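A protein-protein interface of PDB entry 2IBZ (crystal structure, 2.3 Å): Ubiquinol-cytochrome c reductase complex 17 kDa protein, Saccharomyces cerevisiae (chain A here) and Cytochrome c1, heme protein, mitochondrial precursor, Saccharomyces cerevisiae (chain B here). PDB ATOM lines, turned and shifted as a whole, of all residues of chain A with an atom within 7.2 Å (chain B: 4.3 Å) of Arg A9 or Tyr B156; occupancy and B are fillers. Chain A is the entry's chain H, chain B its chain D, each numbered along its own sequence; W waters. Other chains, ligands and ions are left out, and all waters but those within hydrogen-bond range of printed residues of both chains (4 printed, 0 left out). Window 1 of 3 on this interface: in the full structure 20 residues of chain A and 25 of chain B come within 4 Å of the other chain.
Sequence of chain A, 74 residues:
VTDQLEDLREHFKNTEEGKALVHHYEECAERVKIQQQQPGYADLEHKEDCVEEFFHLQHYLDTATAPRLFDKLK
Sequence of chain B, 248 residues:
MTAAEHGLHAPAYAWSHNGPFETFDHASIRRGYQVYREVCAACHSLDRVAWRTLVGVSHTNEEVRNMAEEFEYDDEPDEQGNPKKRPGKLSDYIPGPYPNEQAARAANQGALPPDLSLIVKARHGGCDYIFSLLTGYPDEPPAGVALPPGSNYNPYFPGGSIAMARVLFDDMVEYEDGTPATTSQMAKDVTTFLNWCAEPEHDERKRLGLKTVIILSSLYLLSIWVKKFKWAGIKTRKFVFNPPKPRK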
ATOM      1  N   ASP A   3      11.365  13.116  16.467  1.00  0.00           N
ATOM      2  CA  ASP A   3      12.550  13.887  16.857  1.00  0.00           C
ATOM      3  C   ASP A   3      13.125  13.467  18.207  1.00  0.00           C
ATOM      4  O   ASP A   3      12.420  13.451  19.216  1.00  0.00           O
ATOM      5  CB  ASP A   3      12.269  15.391  16.864  1.00  0.00           C
ATOM      6  CG  ASP A   3      13.494  16.201  17.271  1.00  0.00           C
ATOM      7  OD1 ASP A   3      14.566  15.990  16.663  1.00  0.00           O
ATOM      8  OD2 ASP A   3      13.395  17.021  18.215  1.00  0.00           O
ATOM      9  N   GLN A   4      14.424  13.179  18.210  1.00  0.00           N
ATOM     10  CA  GLN A   4      15.150  12.722  19.389  1.00  0.00           C
ATOM     11  C   GLN A   4      15.218  13.725  20.540  1.00  0.00           C
ATOM     12  O   GLN A   4      15.218  13.337  21.709  1.00  0.00           O
ATOM     13  CB  GLN A   4      16.562  12.291  18.990  1.00  0.00           C
ATOM     14  CG  GLN A   4      16.634  11.145  17.977  1.00  0.00           C
ATOM     15  CD  GLN A   4      16.606  11.593  16.518  1.00  0.00           C
ATOM     16  OE1 GLN A   4      17.087  10.882  15.635  1.00  0.00           O
ATOM     17  NE2 GLN A   4      16.043  12.767  16.260  1.00  0.00           N
ATOM     18  N   LEU A   5      15.293  15.010  20.209  1.00  0.00           N
ATOM     19  CA  LEU A   5      15.357  16.058  21.218  1.00  0.00           C
ATOM     20  C   LEU A   5      13.990  16.234  21.886  1.00  0.00           C
ATOM     21  O   LEU A   5      13.896  16.276  23.117  1.00  0.00           O
ATOM     22  CB  LEU A   5      15.834  17.373  20.588  1.00  0.00           C
ATOM     23  CG  LEU A   5      16.063  18.590  21.489  1.00  0.00           C
ATOM     24  CD1 LEU A   5      17.096  18.291  22.557  1.00  0.00           C
ATOM     25  CD2 LEU A   5      16.516  19.749  20.642  1.00  0.00           C
ATOM     26  N   GLU A   6      12.936  16.325  21.073  1.00  0.00           N
ATOM     27  CA  GLU A   6      11.575  16.477  21.588  1.00  0.00           C
ATOM     28  C   GLU A   6      11.222  15.319  22.503  1.00  0.00           C
ATOM     29  O   GLU A   6      10.494  15.490  23.480  1.00  0.00           O
ATOM     30  CB  GLU A   6      10.555  16.539  20.452  1.00  0.00           C
ATOM     31  CG  GLU A   6      10.457  17.885  19.777  1.00  0.00           C
ATOM     32  CD  GLU A   6       9.033  18.220  19.372  1.00  0.00           C
ATOM     33  OE1 GLU A   6       8.660  17.940  18.209  1.00  0.00           O
ATOM     34  OE2 GLU A   6       8.286  18.756  20.225  1.00  0.00           O
ATOM     35  N   ASP A   7      11.740  14.141  22.166  1.00  0.00           N
ATOM     36  CA  ASP A   7      11.517  12.932  22.943  1.00  0.00           C
ATOM     37  C   ASP A   7      12.115  13.096  24.340  1.00  0.00           C
ATOM     38  O   ASP A   7      11.404  12.979  25.335  1.00  0.00           O
ATOM     39  CB  ASP A   7      12.156  11.738  22.231  1.00  0.00           C
ATOM     40  CG  ASP A   7      11.940  10.429  22.970  1.00  0.00           C
ATOM     41  OD1 ASP A   7      10.943   9.737  22.658  1.00  0.00           O
ATOM     42  OD2 ASP A   7      12.766  10.092  23.852  1.00  0.00           O
ATOM     43  N   LEU A   8      13.417  13.385  24.402  1.00  0.00           N
ATOM     44  CA  LEU A   8      14.119  13.577  25.673  1.00  0.00           C
ATOM     45  C   LEU A   8      13.563  14.739  26.502  1.00  0.00           C
ATOM     46  O   LEU A   8      13.595  14.700  27.734  1.00  0.00           O
ATOM     47  CB  LEU A   8      15.626  13.751  25.438  1.00  0.00           C
ATOM     48  CG  LEU A   8      16.440  12.480  25.185  1.00  0.00           C
ATOM     49  CD1 LEU A   8      17.882  12.834  24.877  1.00  0.00           C
ATOM     50  CD2 LEU A   8      16.376  11.587  26.405  1.00  0.00           C
ATOM     51  N   ARG A   9      13.056  15.773  25.836  1.00  0.00           N
ATOM     52  CA  ARG A   9      12.478  16.904  26.550  1.00  0.00           C
ATOM     53  C   ARG A   9      11.187  16.460  27.231  1.00  0.00           C
ATOM     54  O   ARG A   9      11.061  16.554  28.453  1.00  0.00           O
ATOM     55  CB  ARG A   9      12.234  18.085  25.605  1.00  0.00           C
ATOM     56  CG  ARG A   9      13.490  18.911  25.378  1.00  0.00           C
ATOM     57  CD  ARG A   9      13.318  20.075  24.413  1.00  0.00           C
ATOM     58  NE  ARG A   9      14.537  20.883  24.419  1.00  0.00           N
ATOM     59  CZ  ARG A   9      14.876  21.783  23.499  1.00  0.00           C
ATOM     60  NH1 ARG A   9      16.015  22.449  23.637  1.00  0.00           N
ATOM     61  NH2 ARG A   9      14.092  22.025  22.452  1.00  0.00           N
ATOM     62  N   GLU A  10      10.264  15.911  26.440  1.00  0.00           N
ATOM     63  CA  GLU A  10       8.982  15.419  26.941  1.00  0.00           C
ATOM     64  C   GLU A  10       9.239  14.480  28.116  1.00  0.00           C
ATOM     65  O   GLU A  10       8.633  14.614  29.179  1.00  0.00           O
ATOM     66  CB  GLU A  10       8.220  14.689  25.826  1.00  0.00           C
ATOM     67  CG  GLU A  10       6.721  14.560  26.062  1.00  0.00           C
ATOM     68  CD  GLU A  10       6.041  15.913  26.236  1.00  0.00           C
ATOM     69  OE1 GLU A  10       6.312  16.832  25.424  1.00  0.00           O
ATOM     70  OE2 GLU A  10       5.245  16.064  27.192  1.00  0.00           O
ATOM     71  N   HIS A  11      10.193  13.574  27.940  1.00  0.00           N
ATOM     72  CA  HIS A  11      10.555  12.637  28.988  1.00  0.00           C
ATOM     73  C   HIS A  11      10.947  13.353  30.286  1.00  0.00           C
ATOM     74  O   HIS A  11      10.484  12.971  31.361  1.00  0.00           O
ATOM     75  CB  HIS A  11      11.699  11.740  28.523  1.00  0.00           C
ATOM     76  CG  HIS A  11      12.282  10.898  29.613  1.00  0.00           C
ATOM     77  ND1 HIS A  11      11.712   9.709  30.021  1.00  0.00           N
ATOM     78  CD2 HIS A  11      13.366  11.087  30.403  1.00  0.00           C
ATOM     79  CE1 HIS A  11      12.420   9.203  31.016  1.00  0.00           C
ATOM     80  NE2 HIS A  11      13.429  10.020  31.268  1.00  0.00           N
ATOM     81  N   PHE A  12      11.779  14.395  30.183  1.00  0.00           N
ATOM     82  CA  PHE A  12      12.233  15.133  31.364  1.00  0.00           C
ATOM     83  C   PHE A  12      11.230  16.100  31.973  1.00  0.00           C
ATOM     84  O   PHE A  12      11.282  16.376  33.177  1.00  0.00           O
ATOM     85  CB  PHE A  12      13.600  15.789  31.127  1.00  0.00           C
ATOM     86  CG  PHE A  12      14.750  14.827  31.263  1.00  0.00           C
ATOM     87  CD1 PHE A  12      15.366  14.294  30.139  1.00  0.00           C
ATOM     88  CD2 PHE A  12      15.162  14.392  32.518  1.00  0.00           C
ATOM     89  CE1 PHE A  12      16.373  13.337  30.259  1.00  0.00           C
ATOM     90  CE2 PHE A  12      16.171  13.433  32.651  1.00  0.00           C
ATOM     91  CZ  PHE A  12      16.774  12.904  31.519  1.00  0.00           C
ATOM     92  N   LYS A  13      10.301  16.594  31.159  1.00  0.00           N
ATOM     93  CA  LYS A  13       9.262  17.484  31.670  1.00  0.00           C
ATOM     94  C   LYS A  13       8.367  16.686  32.639  1.00  0.00           C
ATOM     95  O   LYS A  13       7.644  17.267  33.453  1.00  0.00           O
ATOM     96  CB  LYS A  13       8.415  18.038  30.519  1.00  0.00           C
ATOM     97  CG  LYS A  13       9.211  18.826  29.495  1.00  0.00           C
ATOM     98  CD  LYS A  13       8.406  19.166  28.236  1.00  0.00           C
ATOM     99  CE  LYS A  13       7.549  20.413  28.407  1.00  0.00           C
ATOM    100  NZ  LYS A  13       6.498  20.261  29.453  1.00  0.00           N
ATOM    101  N   ASN A  14       8.458  15.355  32.572  1.00  0.00           N
ATOM    102  CA  ASN A  14       7.654  14.472  33.416  1.00  0.00           C
ATOM    103  C   ASN A  14       8.350  13.807  34.600  1.00  0.00           C
ATOM    104  O   ASN A  14       7.859  12.809  35.130  1.00  0.00           O
ATOM    105  CB  ASN A  14       6.927  13.417  32.570  1.00  0.00           C
ATOM    106  CG  ASN A  14       5.745  13.998  31.811  1.00  0.00           C
ATOM    107  OD1 ASN A  14       4.748  14.414  32.412  1.00  0.00           O
ATOM    108  ND2 ASN A  14       5.855  14.046  30.484  1.00  0.00           N
ATOM    109  N   THR A  15       9.508  14.327  34.991  1.00  0.00           N
ATOM    110  CA  THR A  15      10.216  13.802  36.158  1.00  0.00           C
ATOM    111  C   THR A  15       9.699  14.657  37.320  1.00  0.00           C
ATOM    112  O   THR A  15       8.941  15.611  37.101  1.00  0.00           O
ATOM    113  CB  THR A  15      11.750  13.968  36.025  1.00  0.00           C
ATOM    114  OG1 THR A  15      12.068  15.351  35.829  1.00  0.00           O
ATOM    115  CG2 THR A  15      12.283  13.159  34.853  1.00  0.00           C
ATOM    116  N   PHE A  55      12.701  30.191  31.512  1.00  0.00           N
ATOM    117  CA  PHE A  55      14.140  29.944  31.442  1.00  0.00           C
ATOM    118  C   PHE A  55      14.574  28.859  32.429  1.00  0.00           C
ATOM    119  O   PHE A  55      15.427  28.036  32.104  1.00  0.00           O
ATOM    120  CB  PHE A  55      14.938  31.240  31.683  1.00  0.00           C
ATOM    121  CG  PHE A  55      15.203  32.051  30.433  1.00  0.00           C
ATOM    122  CD1 PHE A  55      16.335  32.861  30.347  1.00  0.00           C
ATOM    123  CD2 PHE A  55      14.326  32.025  29.355  1.00  0.00           C
ATOM    124  CE1 PHE A  55      16.593  33.641  29.202  1.00  0.00           C
ATOM    125  CE2 PHE A  55      14.572  32.799  28.204  1.00  0.00           C
ATOM    126  CZ  PHE A  55      15.711  33.610  28.133  1.00  0.00           C
ATOM    127  N   GLN A  58      13.490  25.547  30.805  1.00  0.00           N
ATOM    128  CA  GLN A  58      14.383  25.284  29.684  1.00  0.00           C
ATOM    129  C   GLN A  58      15.800  24.949  30.139  1.00  0.00           C
ATOM    130  O   GLN A  58      16.441  24.055  29.576  1.00  0.00           O
ATOM    131  CB  GLN A  58      14.419  26.479  28.748  1.00  0.00           C
ATOM    132  CG  GLN A  58      14.842  26.107  27.359  1.00  0.00           C
ATOM    133  CD  GLN A  58      13.793  25.284  26.619  1.00  0.00           C
ATOM    134  OE1 GLN A  58      12.615  25.209  27.030  1.00  0.00           O
ATOM    135  NE2 GLN A  58      14.207  24.677  25.509  1.00  0.00           N
ATOM    136  N   HIS A  59      16.278  25.648  31.168  1.00  0.00           N
ATOM    137  CA  HIS A  59      17.617  25.390  31.674  1.00  0.00           C
ATOM    138  C   HIS A  59      17.713  23.963  32.199  1.00  0.00           C
ATOM    139  O   HIS A  59      18.658  23.242  31.872  1.00  0.00           O
ATOM    140  CB  HIS A  59      18.022  26.389  32.763  1.00  0.00           C
ATOM    141  CG  HIS A  59      19.383  26.123  33.329  1.00  0.00           C
ATOM    142  ND1 HIS A  59      20.541  26.338  32.611  1.00  0.00           N
ATOM    143  CD2 HIS A  59      19.768  25.589  34.513  1.00  0.00           C
ATOM    144  CE1 HIS A  59      21.579  25.943  33.326  1.00  0.00           C
ATOM    145  NE2 HIS A  59      21.138  25.485  34.485  1.00  0.00           N
ATOM    146  N   TYR A  60      16.732  23.562  33.006  1.00  0.00           N
ATOM    147  CA  TYR A  60      16.687  22.212  33.563  1.00  0.00           C
ATOM    148  C   TYR A  60      16.686  21.178  32.437  1.00  0.00           C
ATOM    149  O   TYR A  60      17.436  20.198  32.470  1.00  0.00           O
ATOM    150  CB  TYR A  60      15.432  22.031  34.430  1.00  0.00           C
ATOM    151  CG  TYR A  60      15.159  20.584  34.792  1.00  0.00           C
ATOM    152  CD1 TYR A  60      15.937  19.927  35.744  1.00  0.00           C
ATOM    153  CD2 TYR A  60      14.167  19.852  34.123  1.00  0.00           C
ATOM    154  CE1 TYR A  60      15.744  18.581  36.019  1.00  0.00           C
ATOM    155  CE2 TYR A  60      13.970  18.507  34.387  1.00  0.00           C
ATOM    156  CZ  TYR A  60      14.762  17.875  35.334  1.00  0.00           C
ATOM    157  OH  TYR A  60      14.595  16.529  35.576  1.00  0.00           O
ATOM    158  N   LEU A  61      15.843  21.413  31.439  1.00  0.00           N
ATOM    159  CA  LEU A  61      15.747  20.508  30.303  1.00  0.00           C
ATOM    160  C   LEU A  61      17.070  20.418  29.530  1.00  0.00           C
ATOM    161  O   LEU A  61      17.504  19.322  29.161  1.00  0.00           O
ATOM    162  CB  LEU A  61      14.594  20.932  29.385  1.00  0.00           C
ATOM    163  CG  LEU A  61      13.197  20.932  30.030  1.00  0.00           C
ATOM    164  CD1 LEU A  61      12.163  21.462  29.029  1.00  0.00           C
ATOM    165  CD2 LEU A  61      12.826  19.522  30.521  1.00  0.00           C
ATOM    166  N   ASP A  62      17.717  21.566  29.321  1.00  0.00           N
ATOM    167  CA  ASP A  62      18.995  21.622  28.613  1.00  0.00           C
ATOM    168  C   ASP A  62      20.051  20.796  29.343  1.00  0.00           C
ATOM    169  O   ASP A  62      20.750  19.981  28.738  1.00  0.00           O
ATOM    170  CB  ASP A  62      19.487  23.071  28.490  1.00  0.00           C
ATOM    171  CG  ASP A  62      18.780  23.848  27.394  1.00  0.00           C
ATOM    172  OD1 ASP A  62      18.241  23.222  26.461  1.00  0.00           O
ATOM    173  OD2 ASP A  62      18.778  25.099  27.455  1.00  0.00           O
ATOM    174  N   THR A  65      19.066  17.055  28.805  1.00  0.00           N
ATOM    175  CA  THR A  65      19.072  16.569  27.431  1.00  0.00           C
ATOM    176  C   THR A  65      20.411  16.683  26.700  1.00  0.00           C
ATOM    177  O   THR A  65      20.792  15.785  25.947  1.00  0.00           O
ATOM    178  CB  THR A  65      17.989  17.263  26.588  1.00  0.00           C
ATOM    179  OG1 THR A  65      18.264  18.664  26.509  1.00  0.00           O
ATOM    180  CG2 THR A  65      16.621  17.062  27.212  1.00  0.00           C
ATOM    181  N   LEU B   8      19.203  32.892  26.663  1.00  0.00           N
ATOM    182  CA  LEU B   8      19.430  31.651  27.397  1.00  0.00           C
ATOM    183  C   LEU B   8      20.794  31.077  27.057  1.00  0.00           C
ATOM    184  O   LEU B   8      21.179  31.008  25.892  1.00  0.00           O
ATOM    185  CB  LEU B   8      18.361  30.618  27.045  1.00  0.00           C
ATOM    186  CG  LEU B   8      17.769  29.719  28.133  1.00  0.00           C
ATOM    187  CD1 LEU B   8      17.380  28.416  27.507  1.00  0.00           C
ATOM    188  CD2 LEU B   8      18.727  29.478  29.265  1.00  0.00           C
ATOM    189  N   HIS B   9      21.524  30.667  28.082  1.00  0.00           N
ATOM    190  CA  HIS B   9      22.836  30.072  27.899  1.00  0.00           C
ATOM    191  C   HIS B   9      22.667  28.731  27.186  1.00  0.00           C
ATOM    192  O   HIS B   9      21.881  27.889  27.612  1.00  0.00           O
ATOM    193  CB  HIS B   9      23.508  29.861  29.266  1.00  0.00           C
ATOM    194  CG  HIS B   9      24.755  29.029  29.211  1.00  0.00           C
ATOM    195  ND1 HIS B   9      24.803  27.731  29.679  1.00  0.00           N
ATOM    196  CD2 HIS B   9      25.994  29.305  28.734  1.00  0.00           C
ATOM    197  CE1 HIS B   9      26.018  27.242  29.490  1.00  0.00           C
ATOM    198  NE2 HIS B   9      26.760  28.176  28.919  1.00  0.00           N
ATOM    199  N   ALA B  10      23.400  28.547  26.098  1.00  0.00           N
ATOM    200  CA  ALA B  10      23.343  27.309  25.345  1.00  0.00           C
ATOM    201  C   ALA B  10      24.131  26.247  26.102  1.00  0.00           C
ATOM    202  O   ALA B  10      25.208  26.523  26.626  1.00  0.00           O
ATOM    203  CB  ALA B  10      23.919  27.513  23.958  1.00  0.00           C
ATOM    204  N   PRO B  11      23.575  25.025  26.210  1.00  0.00           N
ATOM    205  CA  PRO B  11      24.215  23.907  26.908  1.00  0.00           C
ATOM    206  C   PRO B  11      25.280  23.255  26.039  1.00  0.00           C
ATOM    207  O   PRO B  11      25.312  23.460  24.820  1.00  0.00           O
ATOM    208  CB  PRO B  11      23.046  22.962  27.149  1.00  0.00           C
ATOM    209  CG  PRO B  11      22.256  23.127  25.911  1.00  0.00           C
ATOM    210  CD  PRO B  11      22.254  24.625  25.690  1.00  0.00           C
ATOM    211  N   TYR B 129      25.635  27.049  20.346  1.00  0.00           N
ATOM    212  CA  TYR B 129      24.687  28.134  20.135  1.00  0.00           C
ATOM    213  C   TYR B 129      23.847  27.913  18.886  1.00  0.00           C
ATOM    214  O   TYR B 129      22.635  27.907  18.961  1.00  0.00           O
ATOM    215  CB  TYR B 129      25.408  29.495  20.061  1.00  0.00           C
ATOM    216  CG  TYR B 129      24.515  30.620  19.605  1.00  0.00           C
ATOM    217  CD1 TYR B 129      23.486  31.094  20.426  1.00  0.00           C
ATOM    218  CD2 TYR B 129      24.646  31.166  18.339  1.00  0.00           C
ATOM    219  CE1 TYR B 129      22.603  32.076  19.985  1.00  0.00           C
ATOM    220  CE2 TYR B 129      23.771  32.154  17.887  1.00  0.00           C
ATOM    221  CZ  TYR B 129      22.751  32.600  18.719  1.00  0.00           C
ATOM    222  OH  TYR B 129      21.873  33.562  18.283  1.00  0.00           O
ATOM    223  N   SER B 132      21.439  24.952  19.266  1.00  0.00           N
ATOM    224  CA  SER B 132      20.385  25.314  20.194  1.00  0.00           C
ATOM    225  C   SER B 132      19.393  26.297  19.603  1.00  0.00           C
ATOM    226  O   SER B 132      18.194  26.166  19.808  1.00  0.00           O
ATOM    227  CB  SER B 132      20.981  25.856  21.490  1.00  0.00           C
ATOM    228  OG  SER B 132      21.632  24.822  22.216  1.00  0.00           O
ATOM    229  N   THR B 135      17.004  24.466  17.127  1.00  0.00           N
ATOM    230  CA  THR B 135      16.121  23.502  17.754  1.00  0.00           C
ATOM    231  C   THR B 135      15.402  24.097  18.962  1.00  0.00           C
ATOM    232  O   THR B 135      14.709  23.387  19.696  1.00  0.00           O
ATOM    233  CB  THR B 135      16.932  22.303  18.245  1.00  0.00           C
ATOM    234  OG1 THR B 135      17.947  22.760  19.147  1.00  0.00           O
ATOM    235  CG2 THR B 135      17.588  21.585  17.082  1.00  0.00           C
ATOM    236  N   GLY B 136      15.540  25.402  19.154  1.00  0.00           N
ATOM    237  CA  GLY B 136      14.941  26.026  20.314  1.00  0.00           C
ATOM    238  C   GLY B 136      13.738  26.916  20.133  1.00  0.00           C
ATOM    239  O   GLY B 136      13.481  27.742  20.999  1.00  0.00           O
ATOM    240  N   ASN B 154      12.578  32.963  20.405  1.00  0.00           N
ATOM    241  CA  ASN B 154      13.605  31.943  20.558  1.00  0.00           C
ATOM    242  C   ASN B 154      14.334  32.374  21.815  1.00  0.00           C
ATOM    243  O   ASN B 154      14.886  33.476  21.873  1.00  0.00           O
ATOM    244  CB  ASN B 154      14.555  31.953  19.365  1.00  0.00           C
ATOM    245  CG  ASN B 154      15.397  30.710  19.296  1.00  0.00           C
ATOM    246  OD1 ASN B 154      16.076  30.351  20.262  1.00  0.00           O
ATOM    247  ND2 ASN B 154      15.350  30.027  18.160  1.00  0.00           N
ATOM    248  N   PRO B 155      14.347  31.518  22.846  1.00  0.00           N
ATOM    249  CA  PRO B 155      15.011  31.844  24.111  1.00  0.00           C
ATOM    250  C   PRO B 155      16.533  32.024  24.036  1.00  0.00           C
ATOM    251  O   PRO B 155      17.108  32.765  24.830  1.00  0.00           O
ATOM    252  CB  PRO B 155      14.617  30.670  25.000  1.00  0.00           C
ATOM    253  CG  PRO B 155      14.626  29.532  24.033  1.00  0.00           C
ATOM    254  CD  PRO B 155      13.902  30.115  22.839  1.00  0.00           C
ATOM    255  N   TYR B 156      17.181  31.375  23.075  1.00  0.00           N
ATOM    256  CA  TYR B 156      18.636  31.465  22.938  1.00  0.00           C
ATOM    257  C   TYR B 156      19.168  32.735  22.275  1.00  0.00           C
ATOM    258  O   TYR B 156      20.335  33.065  22.427  1.00  0.00           O
ATOM    259  CB  TYR B 156      19.168  30.222  22.234  1.00  0.00           C
ATOM    260  CG  TYR B 156      18.806  28.956  22.969  1.00  0.00           C
ATOM    261  CD1 TYR B 156      17.710  28.187  22.573  1.00  0.00           C
ATOM    262  CD2 TYR B 156      19.534  28.541  24.084  1.00  0.00           C
ATOM    263  CE1 TYR B 156      17.345  27.034  23.274  1.00  0.00           C
ATOM    264  CE2 TYR B 156      19.180  27.392  24.791  1.00  0.00           C
ATOM    265  CZ  TYR B 156      18.077  26.644  24.372  1.00  0.00           C
ATOM    266  OH  TYR B 156      17.712  25.515  25.054  1.00  0.00           O
ATOM    267  N   PHE B 157      18.306  33.451  21.559  1.00  0.00           N
ATOM    268  CA  PHE B 157      18.683  34.688  20.890  1.00  0.00           C
ATOM    269  C   PHE B 157      18.530  35.839  21.896  1.00  0.00           C
ATOM    270  O   PHE B 157      17.545  35.889  22.637  1.00  0.00           O
ATOM    271  CB  PHE B 157      17.754  34.918  19.700  1.00  0.00           C
ATOM    272  CG  PHE B 157      18.192  36.027  18.783  1.00  0.00           C
ATOM    273  CD1 PHE B 157      19.350  35.896  18.009  1.00  0.00           C
ATOM    274  CD2 PHE B 157      17.445  37.199  18.682  1.00  0.00           C
ATOM    275  CE1 PHE B 157      19.756  36.925  17.140  1.00  0.00           C
ATOM    276  CE2 PHE B 157      17.837  38.230  17.826  1.00  0.00           C
ATOM    277  CZ  PHE B 157      18.996  38.097  17.048  1.00  0.00           C
ATOM    278  N   PRO B 158      19.521  36.752  21.966  1.00  0.00           N
ATOM    279  CA  PRO B 158      19.477  37.893  22.895  1.00  0.00           C
ATOM    280  C   PRO B 158      18.250  38.734  22.636  1.00  0.00           C
ATOM    281  O   PRO B 158      18.023  39.165  21.511  1.00  0.00           O
ATOM    282  CB  PRO B 158      20.750  38.665  22.546  1.00  0.00           C
ATOM    283  CG  PRO B 158      21.695  37.571  22.136  1.00  0.00           C
ATOM    284  CD  PRO B 158      20.809  36.714  21.248  1.00  0.00           C
HETATM  285  O   HOH W   1      19.277  23.419  23.458  1.00  0.00           O
HETATM  286  O   HOH W   2      20.843  25.924  29.113  1.00  0.00           O
HETATM  287  O   HOH W   3      12.939  26.545  23.419  1.00  0.00           O
HETATM  288  O   HOH W   4      17.440  24.182  21.430  1.00  0.00           O
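O of Thr B135 sits at hydrogen-bond distance from NH2 of Arg A9, 3.1 Å away. The side-chain carboxylate of Asp A62 lies within hydrogen-bond range of the side-chain hydroxyl of Tyr B156 (2.7 Å).
The backbone carbonyl oxygen of Pro B155 sits at hydrogen-bond distance from the backbone NH of Leu B8 (2.8 Å). O of Ser B132 sits at hydrogen-bond distance from OG1 of Thr B135, 3.5 Å away. OD1 of Asn B154 lies within hydrogen-bond range of N of Tyr B156. The side-chain carboxylate (OD2) of Asp A3 sits close to the backbone NH (N) of Leu A5 (3.4 Å). The guanidinium group (NH1) of Arg A9 lies close to the side-chain amide nitrogen (NE2) of Gln A58 (3.4 Å). NH1 of Arg A9 is in salt-bridge range of OD1 of Asp A62 (3.7 Å).
Thr B135 touches Leu A5 (CB to CD2, 3.5 Å). Tyr B156 touches Arg A9. Leu B8 touches Phe A55. CZ of Phe A55 touches O of Pro B155, 3.7 Å away. Gln A58 touches Leu B8 (CG to CD1, 3.4 Å). Gln A58 touches Tyr B156 (NE2 to OH, 3.6 Å). OD2 of Asp A62 touches CD1 of Leu B8, at 3.6 Å. CG of Pro B11 touches CB of Asp A62 (3.8 Å).
Of the printed residues of chain B, Leu A5 touches Thr B135. Arg A9 touches just these residues of chain B: Thr B135 (3.1 Å) and Tyr B156 (3.8 Å). Of the printed residues of chain B, Gln A58 touches Leu B8 (3.4 Å) and Tyr B156 (3.6 Å). Thr A65 touches none of the printed residues of chain B. Of the printed residues of chain A, Leu B8 touches Phe A55, Gln A58 and Asp A62. Of the printed residues of chain A, Pro B11 touches Asp A62. Ser B132 touches none of the printed residues of chain A. Of chain A, only Arg A9, Gln A58 and Asp A62 come within 4 Å of Tyr B156. The nearest residue of chain A that does not touch Tyr B156 is Phe A55 (5.7 Å).
Hydrophobic or aromatic side chains of chain A within 4 Å of the printed part of chain B: Leu A5 and Phe A55. Among the printed residues, no Asp or Glu carboxylate lies within 4 Å of a Lys or Arg side-chain nitrogen of the other chain.
Water W4 lies within hydrogen-bond range of the backbone carbonyl oxygen (O) of Ser B132, the side-chain hydroxyl (OG1) of Thr B135, the guanidinium group (NH1) of Arg A9 and the backbone NH (N) of Gly B136. Water W2 bridges O of His B9 (2.7 Å) and OD2 of Asp A62 (2.8 Å). Water W3 bridges the backbone carbonyl oxygen of Gly B136 (2.8 Å) and the side-chain amide nitrogen of Gln A58 (3.1 Å). Water W1 lies within hydrogen-bond range of the side-chain hydroxyl of Ser B132 (3.0 Å), the side-chain hydroxyl of Tyr B156 (3.1 Å), the side-chain carboxylate of Asp A62 (3.2 Å) and the guanidinium group of Arg A9 (3.4 Å).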
